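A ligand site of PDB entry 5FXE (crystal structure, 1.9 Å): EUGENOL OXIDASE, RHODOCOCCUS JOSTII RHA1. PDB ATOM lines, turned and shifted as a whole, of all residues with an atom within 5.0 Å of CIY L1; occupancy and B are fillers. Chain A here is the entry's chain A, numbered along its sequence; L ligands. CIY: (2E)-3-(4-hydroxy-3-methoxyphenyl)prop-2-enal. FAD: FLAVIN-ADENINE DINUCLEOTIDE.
OE1 of Gln 425 sits at hydrogen-bond distance from NH1 of Arg 278 (2.7 Å). OH of Tyr 168 is in hydrogen-bond range of NE2 of Gln 425 (3.0 Å). The guanidinium group (NH2) of Arg 366 lies within salt-bridge range of the side-chain carboxylate (OD1) of Asp 151 (3.0 Å). The backbone NH (N) of Tyr 471 is in hydrogen-bond range of the backbone carbonyl oxygen (O) of Ser 394, 3.0 Å away. The side-chain hydroxyl (OH) of Tyr 471 is in hydrogen-bond range of the guanidinium group (NH1) of Arg 472, 3.0 Å away. The backbone NH (N) of Gln 425 lies within hydrogen-bond range of the backbone carbonyl oxygen (O) of Val 436 (2.8 Å). The side-chain carboxylate (OE1) of Glu 378 lies within salt-bridge range of the guanidinium group (NH1) of Arg 278 (2.8 Å). The side-chain hydroxyl of Tyr 91 is in hydrogen-bond range of the side-chain hydroxyl of Ser 394 (2.9 Å).
OE1 of Glu 378 sits close to O9 of CIY L1 (2.6 Å). An oxygen (O2) of FAD L2 lies within hydrogen-bond range of the backbone NH (N) of Val 166 (2.8 Å). The side-chain hydroxyl (OH) of Tyr 471 is in hydrogen-bond range of an oxygen (O4) of CIY L1 (2.5 Å). An oxygen (O4) of FAD L2 is in hydrogen-bond range of the backbone NH of Asp 151 (3.0 Å). A ring nitrogen (NE2) of His 390 is bonded to a carbon (C8M) of FAD L2 (1.4 Å). OH of Tyr 91 sits at hydrogen-bond distance from O4 of CIY L1, at 2.5 Å. O of Val 166 sits at hydrogen-bond distance from N3 of FAD L2 (2.8 Å). An oxygen (O3') of FAD L2 sits at hydrogen-bond distance from the guanidinium group (NH2) of Arg 472 (2.8 Å). The side-chain hydroxyl (OH) of Tyr 168 lies within hydrogen-bond range of an oxygen (O4) of FAD L2. The side-chain carboxylate (OD2) of Asp 151 lies close to an oxygen (O9) of CIY L1 (2.7 Å).
Merely in contact with CIY L1: Gln 425, Val 436, Ile 427, His 390, Arg 472, Tyr 168, Leu 438, Leu 381 and Arg 278. Of the 20 residues printed, 13 come within 4 Å of CIY L1.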
ATOM      1  N   ASN A  89      21.482  -4.207   8.832  1.00  0.00           N
ATOM      2  CA  ASN A  89      22.854  -3.782   8.959  1.00  0.00           C
ATOM      3  C   ASN A  89      23.460  -4.255  10.230  1.00  0.00           C
ATOM      4  O   ASN A  89      22.887  -4.168  11.340  1.00  0.00           O
ATOM      5  CB  ASN A  89      22.915  -2.266   8.834  1.00  0.00           C
ATOM      6  CG  ASN A  89      22.358  -1.770   7.505  1.00  0.00           C
ATOM      7  OD1 ASN A  89      22.187  -2.523   6.543  1.00  0.00           O
ATOM      8  ND2 ASN A  89      22.127  -0.495   7.439  1.00  0.00           N
ATOM      9  N   GLY A  90      24.636  -4.838  10.082  1.00  0.00           N
ATOM     10  CA  GLY A  90      25.315  -5.479  11.170  1.00  0.00           C
ATOM     11  C   GLY A  90      25.253  -6.977  10.954  1.00  0.00           C
ATOM     12  O   GLY A  90      26.062  -7.700  11.549  1.00  0.00           O
ATOM     13  N   TYR A  91      24.298  -7.420  10.181  1.00  0.00           N
ATOM     14  CA  TYR A  91      24.086  -8.846   9.941  1.00  0.00           C
ATOM     15  C   TYR A  91      24.064  -9.205   8.483  1.00  0.00           C
ATOM     16  O   TYR A  91      23.827 -10.383   8.102  1.00  0.00           O
ATOM     17  CB  TYR A  91      22.843  -9.320  10.649  1.00  0.00           C
ATOM     18  CG  TYR A  91      22.858  -9.186  12.141  1.00  0.00           C
ATOM     19  CD1 TYR A  91      23.832  -9.746  12.888  1.00  0.00           C
ATOM     20  CD2 TYR A  91      21.857  -8.470  12.807  1.00  0.00           C
ATOM     21  CE1 TYR A  91      23.814  -9.661  14.263  1.00  0.00           C
ATOM     22  CE2 TYR A  91      21.807  -8.350  14.201  1.00  0.00           C
ATOM     23  CZ  TYR A  91      22.779  -8.970  14.949  1.00  0.00           C
ATOM     24  OH  TYR A  91      22.747  -8.841  16.328  1.00  0.00           O
ATOM     25  N   ASP A 151      16.730   0.485  18.038  1.00  0.00           N
ATOM     26  CA  ASP A 151      17.574   1.686  18.022  1.00  0.00           C
ATOM     27  C   ASP A 151      17.463   2.558  16.795  1.00  0.00           C
ATOM     28  O   ASP A 151      17.588   3.761  16.933  1.00  0.00           O
ATOM     29  CB  ASP A 151      19.033   1.282  18.250  1.00  0.00           C
ATOM     30  CG  ASP A 151      19.317   1.047  19.708  1.00  0.00           C
ATOM     31  OD1 ASP A 151      18.342   1.111  20.449  1.00  0.00           O
ATOM     32  OD2 ASP A 151      20.450   0.829  20.165  1.00  0.00           O
ATOM     33  N   VAL A 166      14.934  -6.918  18.652  1.00  0.00           N
ATOM     34  CA  VAL A 166      14.541  -6.491  19.980  1.00  0.00           C
ATOM     35  C   VAL A 166      14.396  -5.015  20.036  1.00  0.00           C
ATOM     36  O   VAL A 166      15.107  -4.240  19.300  1.00  0.00           O
ATOM     37  CB  VAL A 166      15.544  -6.949  21.033  1.00  0.00           C
ATOM     38  CG1 VAL A 166      15.618  -8.470  21.143  1.00  0.00           C
ATOM     39  CG2 VAL A 166      16.957  -6.438  20.715  1.00  0.00           C
ATOM     40  N   TYR A 168      12.875  -1.986  23.350  1.00  0.00           N
ATOM     41  CA  TYR A 168      13.207  -1.571  24.707  1.00  0.00           C
ATOM     42  C   TYR A 168      12.073  -1.150  25.650  1.00  0.00           C
ATOM     43  O   TYR A 168      12.334  -0.855  26.834  1.00  0.00           O
ATOM     44  CB  TYR A 168      14.268  -0.483  24.655  1.00  0.00           C
ATOM     45  CG  TYR A 168      15.430  -0.935  23.797  1.00  0.00           C
ATOM     46  CD1 TYR A 168      16.427  -1.723  24.344  1.00  0.00           C
ATOM     47  CD2 TYR A 168      15.482  -0.651  22.459  1.00  0.00           C
ATOM     48  CE1 TYR A 168      17.443  -2.233  23.584  1.00  0.00           C
ATOM     49  CE2 TYR A 168      16.511  -1.110  21.661  1.00  0.00           C
ATOM     50  CZ  TYR A 168      17.525  -1.912  22.214  1.00  0.00           C
ATOM     51  OH  TYR A 168      18.578  -2.460  21.446  1.00  0.00           O
ATOM     52  N   ARG A 278      25.484  -0.170  28.528  1.00  0.00           N
ATOM     53  CA  ARG A 278      26.312   0.213  27.416  1.00  0.00           C
ATOM     54  C   ARG A 278      27.710   0.601  27.957  1.00  0.00           C
ATOM     55  O   ARG A 278      27.830   1.195  29.021  1.00  0.00           O
ATOM     56  CB  ARG A 278      25.700   1.366  26.629  1.00  0.00           C
ATOM     57  CG  ARG A 278      24.485   0.925  25.826  1.00  0.00           C
ATOM     58  CD  ARG A 278      23.513   2.037  25.431  1.00  0.00           C
ATOM     59  NE  ARG A 278      24.182   3.018  24.632  1.00  0.00           N
ATOM     60  CZ  ARG A 278      24.073   3.190  23.313  1.00  0.00           C
ATOM     61  NH1 ARG A 278      23.272   2.439  22.559  1.00  0.00           N
ATOM     62  NH2 ARG A 278      24.736   4.180  22.746  1.00  0.00           N
ATOM     63  N   MET A 282      30.635   2.448  23.267  1.00  0.00           N
ATOM     64  CA  MET A 282      29.312   2.551  22.637  1.00  0.00           C
ATOM     65  C   MET A 282      28.859   3.962  22.754  1.00  0.00           C
ATOM     66  O   MET A 282      28.497   4.617  21.759  1.00  0.00           O
ATOM     67  CB  MET A 282      28.307   1.572  23.314  1.00  0.00           C
ATOM     68  CG  MET A 282      26.993   1.402  22.586  1.00  0.00           C
ATOM     69  SD  MET A 282      27.048   0.743  20.917  1.00  0.00           S
ATOM     70  CE  MET A 282      27.142  -1.012  21.306  1.00  0.00           C
ATOM     71  N   ARG A 366      17.642   7.333  24.402  1.00  0.00           N
ATOM     72  CA  ARG A 366      17.000   6.201  25.064  1.00  0.00           C
ATOM     73  C   ARG A 366      15.576   6.571  25.552  1.00  0.00           C
ATOM     74  O   ARG A 366      14.676   5.798  25.411  1.00  0.00           O
ATOM     75  CB  ARG A 366      17.793   5.656  26.224  1.00  0.00           C
ATOM     76  CG  ARG A 366      19.236   5.228  25.978  1.00  0.00           C
ATOM     77  CD  ARG A 366      19.564   4.601  24.620  1.00  0.00           C
ATOM     78  NE  ARG A 366      18.940   3.303  24.484  1.00  0.00           N
ATOM     79  CZ  ARG A 366      19.121   2.463  23.460  1.00  0.00           C
ATOM     80  NH1 ARG A 366      19.935   2.791  22.471  1.00  0.00           N
ATOM     81  NH2 ARG A 366      18.480   1.286  23.411  1.00  0.00           N
ATOM     82  N   GLU A 378      21.476   6.842  16.641  1.00  0.00           N
ATOM     83  CA  GLU A 378      22.524   5.853  16.721  1.00  0.00           C
ATOM     84  C   GLU A 378      23.298   5.635  15.399  1.00  0.00           C
ATOM     85  O   GLU A 378      24.284   5.008  15.450  1.00  0.00           O
ATOM     86  CB  GLU A 378      21.988   4.531  17.309  1.00  0.00           C
ATOM     87  CG  GLU A 378      21.709   4.548  18.824  1.00  0.00           C
ATOM     88  CD  GLU A 378      22.969   4.435  19.708  1.00  0.00           C
ATOM     89  OE1 GLU A 378      23.505   3.298  19.882  1.00  0.00           O
ATOM     90  OE2 GLU A 378      23.429   5.477  20.290  1.00  0.00           O
ATOM     91  N   LEU A 381      27.112   6.312  15.480  1.00  0.00           N
ATOM     92  CA  LEU A 381      28.165   5.339  15.827  1.00  0.00           C
ATOM     93  C   LEU A 381      29.068   5.066  14.681  1.00  0.00           C
ATOM     94  O   LEU A 381      30.226   4.803  14.924  1.00  0.00           O
ATOM     95  CB  LEU A 381      27.585   3.993  16.250  1.00  0.00           C
ATOM     96  CG  LEU A 381      26.701   4.002  17.483  1.00  0.00           C
ATOM     97  CD1 LEU A 381      25.770   2.792  17.436  1.00  0.00           C
ATOM     98  CD2 LEU A 381      27.570   4.001  18.702  1.00  0.00           C
ATOM     99  N   HIS A 390      29.640  -1.690  11.087  1.00  0.00           N
ATOM    100  CA  HIS A 390      29.680  -2.546  12.277  1.00  0.00           C
ATOM    101  C   HIS A 390      29.209  -3.975  11.912  1.00  0.00           C
ATOM    102  O   HIS A 390      28.603  -4.220  10.899  1.00  0.00           O
ATOM    103  CB  HIS A 390      28.904  -1.941  13.421  1.00  0.00           C
ATOM    104  CG  HIS A 390      27.397  -1.949  13.258  1.00  0.00           C
ATOM    105  ND1 HIS A 390      26.636  -3.086  13.292  1.00  0.00           N
ATOM    106  CD2 HIS A 390      26.515  -0.940  13.121  1.00  0.00           C
ATOM    107  CE1 HIS A 390      25.352  -2.776  13.215  1.00  0.00           C
ATOM    108  NE2 HIS A 390      25.242  -1.477  13.011  1.00  0.00           N
ATOM    109  N   GLY A 392      27.516  -7.238  14.385  1.00  0.00           N
ATOM    110  CA  GLY A 392      27.051  -7.654  15.703  1.00  0.00           C
ATOM    111  C   GLY A 392      27.468  -9.099  15.989  1.00  0.00           C
ATOM    112  O   GLY A 392      27.052 -10.052  15.283  1.00  0.00           O
ATOM    113  N   SER A 394      26.739 -11.455  18.921  1.00  0.00           N
ATOM    114  CA  SER A 394      25.557 -11.308  19.830  1.00  0.00           C
ATOM    115  C   SER A 394      25.265 -12.510  20.684  1.00  0.00           C
ATOM    116  O   SER A 394      24.164 -13.092  20.584  1.00  0.00           O
ATOM    117  CB  SER A 394      24.354 -10.853  19.024  1.00  0.00           C
ATOM    118  OG  SER A 394      24.741  -9.678  18.311  1.00  0.00           O
ATOM    119  N   GLN A 425      26.639  -3.569  24.302  1.00  0.00           N
ATOM    120  CA  GLN A 425      25.300  -3.227  24.810  1.00  0.00           C
ATOM    121  C   GLN A 425      24.626  -4.487  25.304  1.00  0.00           C
ATOM    122  O   GLN A 425      24.191  -5.314  24.428  1.00  0.00           O
ATOM    123  CB  GLN A 425      24.447  -2.533  23.753  1.00  0.00           C
ATOM    124  CG  GLN A 425      22.998  -2.246  24.170  1.00  0.00           C
ATOM    125  CD  GLN A 425      22.315  -1.246  23.275  1.00  0.00           C
ATOM    126  OE1 GLN A 425      22.790  -0.129  23.148  1.00  0.00           O
ATOM    127  NE2 GLN A 425      21.210  -1.617  22.659  1.00  0.00           N
ATOM    128  N   ILE A 427      21.449  -6.116  26.568  1.00  0.00           N
ATOM    129  CA  ILE A 427      20.010  -5.855  26.468  1.00  0.00           C
ATOM    130  C   ILE A 427      19.307  -6.825  27.392  1.00  0.00           C
ATOM    131  O   ILE A 427      19.408  -8.039  27.197  1.00  0.00           O
ATOM    132  CB  ILE A 427      19.527  -6.012  25.052  1.00  0.00           C
ATOM    133  CG1 ILE A 427      20.346  -5.117  24.150  1.00  0.00           C
ATOM    134  CG2 ILE A 427      18.001  -5.714  24.972  1.00  0.00           C
ATOM    135  CD1 ILE A 427      20.335  -5.561  22.729  1.00  0.00           C
ATOM    136  N   VAL A 436      25.200  -7.661  23.096  1.00  0.00           N
ATOM    137  CA  VAL A 436      25.522  -7.237  21.757  1.00  0.00           C
ATOM    138  C   VAL A 436      26.904  -6.602  21.745  1.00  0.00           C
ATOM    139  O   VAL A 436      27.137  -5.664  22.439  1.00  0.00           O
ATOM    140  CB  VAL A 436      24.465  -6.331  21.144  1.00  0.00           C
ATOM    141  CG1 VAL A 436      24.897  -5.834  19.759  1.00  0.00           C
ATOM    142  CG2 VAL A 436      23.123  -7.089  21.035  1.00  0.00           C
ATOM    143  N   LEU A 438      29.280  -4.791  19.453  1.00  0.00           N
ATOM    144  CA  LEU A 438      29.256  -4.138  18.187  1.00  0.00           C
ATOM    145  C   LEU A 438      30.694  -3.736  17.912  1.00  0.00           C
ATOM    146  O   LEU A 438      31.283  -3.057  18.697  1.00  0.00           O
ATOM    147  CB  LEU A 438      28.365  -2.905  18.297  1.00  0.00           C
ATOM    148  CG  LEU A 438      27.614  -2.489  17.091  1.00  0.00           C
ATOM    149  CD1 LEU A 438      26.651  -3.593  16.690  1.00  0.00           C
ATOM    150  CD2 LEU A 438      26.899  -1.129  17.242  1.00  0.00           C
ATOM    151  N   TYR A 471      22.360 -15.223  19.580  1.00  0.00           N
ATOM    152  CA  TYR A 471      20.906 -15.155  19.318  1.00  0.00           C
ATOM    153  C   TYR A 471      20.589 -14.841  17.846  1.00  0.00           C
ATOM    154  O   TYR A 471      19.500 -15.049  17.371  1.00  0.00           O
ATOM    155  CB  TYR A 471      20.266 -14.148  20.269  1.00  0.00           C
ATOM    156  CG  TYR A 471      19.992 -12.746  19.684  1.00  0.00           C
ATOM    157  CD1 TYR A 471      20.957 -11.782  19.642  1.00  0.00           C
ATOM    158  CD2 TYR A 471      18.741 -12.411  19.203  1.00  0.00           C
ATOM    159  CE1 TYR A 471      20.699 -10.507  19.087  1.00  0.00           C
ATOM    160  CE2 TYR A 471      18.469 -11.175  18.665  1.00  0.00           C
ATOM    161  CZ  TYR A 471      19.442 -10.221  18.594  1.00  0.00           C
ATOM    162  OH  TYR A 471      19.138  -9.010  18.067  1.00  0.00           O
ATOM    163  N   ARG A 472      21.573 -14.326  17.129  1.00  0.00           N
ATOM    164  CA  ARG A 472      21.395 -13.772  15.809  1.00  0.00           C
ATOM    165  C   ARG A 472      22.775 -13.518  15.250  1.00  0.00           C
ATOM    166  O   ARG A 472      23.667 -13.237  16.067  1.00  0.00           O
ATOM    167  CB  ARG A 472      20.680 -12.413  15.959  1.00  0.00           C
ATOM    168  CG  ARG A 472      20.182 -11.788  14.692  1.00  0.00           C
ATOM    169  CD  ARG A 472      19.327 -10.622  15.168  1.00  0.00           C
ATOM    170  NE  ARG A 472      18.830  -9.844  14.079  1.00  0.00           N
ATOM    171  CZ  ARG A 472      18.283  -8.629  14.218  1.00  0.00           C
ATOM    172  NH1 ARG A 472      18.096  -8.061  15.394  1.00  0.00           N
ATOM    173  NH2 ARG A 472      17.943  -7.986  13.157  1.00  0.00           N
HETATM  174  C1  CIY L   1      21.765  -3.570  18.644  1.00  0.00           C
HETATM  175  C2  CIY L   1      22.407  -4.088  17.504  1.00  0.00           C
HETATM  176  C3  CIY L   1      22.191  -5.392  17.111  1.00  0.00           C
HETATM  177  O3  CIY L   1      22.732  -5.973  16.000  1.00  0.00           O
HETATM  178  C4  CIY L   1      21.293  -6.181  17.844  1.00  0.00           C
HETATM  179  O4  CIY L   1      21.017  -7.475  17.472  1.00  0.00           O
HETATM  180  C5  CIY L   1      20.622  -5.625  18.941  1.00  0.00           C
HETATM  181  C6  CIY L   1      20.878  -4.360  19.349  1.00  0.00           C
HETATM  182  C7  CIY L   1      21.987  -2.293  19.156  1.00  0.00           C
HETATM  183  C8  CIY L   1      23.041  -1.532  18.927  1.00  0.00           C
HETATM  184  C9  CIY L   1      23.289  -0.241  19.672  1.00  0.00           C
HETATM  185  O9  CIY L   1      22.843   0.973  19.029  1.00  0.00           O
HETATM  186  C3M CIY L   1      23.759  -5.331  15.242  1.00  0.00           C
HETATM  187  PA  FAD L   2      15.076  -6.848   6.970  1.00  0.00           P
HETATM  188  O1A FAD L   2      16.485  -6.595   6.539  1.00  0.00           O
HETATM  189  O2A FAD L   2      14.067  -6.550   5.896  1.00  0.00           O
HETATM  190  O5B FAD L   2      14.956  -8.401   7.265  1.00  0.00           O
HETATM  191  C5B FAD L   2      15.778  -9.103   8.194  1.00  0.00           C
HETATM  192  C4B FAD L   2      15.747 -10.588   7.808  1.00  0.00           C
HETATM  193  O4B FAD L   2      14.468 -11.126   8.132  1.00  0.00           O
HETATM  194  C3B FAD L   2      15.897 -10.909   6.348  1.00  0.00           C
HETATM  195  O3B FAD L   2      17.284 -10.913   6.031  1.00  0.00           O
HETATM  196  C2B FAD L   2      15.272 -12.247   6.190  1.00  0.00           C
HETATM  197  O2B FAD L   2      16.139 -13.196   6.789  1.00  0.00           O
HETATM  198  C1B FAD L   2      14.103 -12.051   7.093  1.00  0.00           C
HETATM  199  N9A FAD L   2      12.948 -11.469   6.408  1.00  0.00           N
HETATM  200  C8A FAD L   2      12.621 -10.157   6.391  1.00  0.00           C
HETATM  201  N7A FAD L   2      11.497  -9.950   5.725  1.00  0.00           N
HETATM  202  C5A FAD L   2      11.078 -11.165   5.374  1.00  0.00           C
HETATM  203  C6A FAD L   2       9.930 -11.634   4.638  1.00  0.00           C
HETATM  204  N6A FAD L   2       9.024 -10.746   4.196  1.00  0.00           N
HETATM  205  N1A FAD L   2       9.821 -12.971   4.465  1.00  0.00           N
HETATM  206  C2A FAD L   2      10.759 -13.805   4.939  1.00  0.00           C
HETATM  207  N3A FAD L   2      11.860 -13.456   5.585  1.00  0.00           N
HETATM  208  C4A FAD L   2      12.015 -12.153   5.849  1.00  0.00           C
HETATM  209  N1  FAD L   2      18.428  -4.647  15.808  1.00  0.00           N
HETATM  210  C2  FAD L   2      17.508  -4.823  16.819  1.00  0.00           C
HETATM  211  O2  FAD L   2      16.738  -5.822  16.784  1.00  0.00           O
HETATM  212  N3  FAD L   2      17.421  -3.969  17.802  1.00  0.00           N
HETATM  213  C4  FAD L   2      18.212  -2.875  17.897  1.00  0.00           C
HETATM  214  O4  FAD L   2      18.153  -2.046  18.848  1.00  0.00           O
HETATM  215  C4X FAD L   2      19.217  -2.644  16.863  1.00  0.00           C
HETATM  216  N5  FAD L   2      20.072  -1.604  16.960  1.00  0.00           N
HETATM  217  C5X FAD L   2      20.950  -1.428  15.913  1.00  0.00           C
HETATM  218  C6  FAD L   2      21.850  -0.394  15.942  1.00  0.00           C
HETATM  219  C7  FAD L   2      22.823  -0.177  14.928  1.00  0.00           C
HETATM  220  C7M FAD L   2      23.715   1.026  15.078  1.00  0.00           C
HETATM  221  C8  FAD L   2      22.905  -1.073  13.784  1.00  0.00           C
HETATM  222  C8M FAD L   2      23.986  -0.932  12.641  1.00  0.00           C
HETATM  223  C9  FAD L   2      21.980  -2.134  13.779  1.00  0.00           C
HETATM  224  C9A FAD L   2      21.063  -2.350  14.760  1.00  0.00           C
HETATM  225  N10 FAD L   2      20.180  -3.459  14.728  1.00  0.00           N
HETATM  226  C10 FAD L   2      19.299  -3.615  15.795  1.00  0.00           C
HETATM  227  C1' FAD L   2      20.153  -4.416  13.610  1.00  0.00           C
HETATM  228  C2' FAD L   2      19.175  -3.949  12.491  1.00  0.00           C
HETATM  229  O2' FAD L   2      19.246  -2.568  12.170  1.00  0.00           O
HETATM  230  C3' FAD L   2      17.668  -3.994  12.840  1.00  0.00           C
HETATM  231  O3' FAD L   2      17.289  -5.244  13.398  1.00  0.00           O
HETATM  232  C4' FAD L   2      16.787  -3.734  11.601  1.00  0.00           C
HETATM  233  O4' FAD L   2      15.461  -3.412  12.061  1.00  0.00           O
HETATM  234  C5' FAD L   2      16.668  -5.012  10.722  1.00  0.00           C
HETATM  235  O5' FAD L   2      16.416  -4.706   9.337  1.00  0.00           O
HETATM  236  P   FAD L   2      14.960  -4.657   8.681  1.00  0.00           P
HETATM  237  O1P FAD L   2      15.012  -3.878   7.430  1.00  0.00           O
HETATM  238  O2P FAD L   2      14.044  -4.338   9.769  1.00  0.00           O
HETATM  239  O3P FAD L   2      14.778  -6.221   8.423  1.00  0.00           O
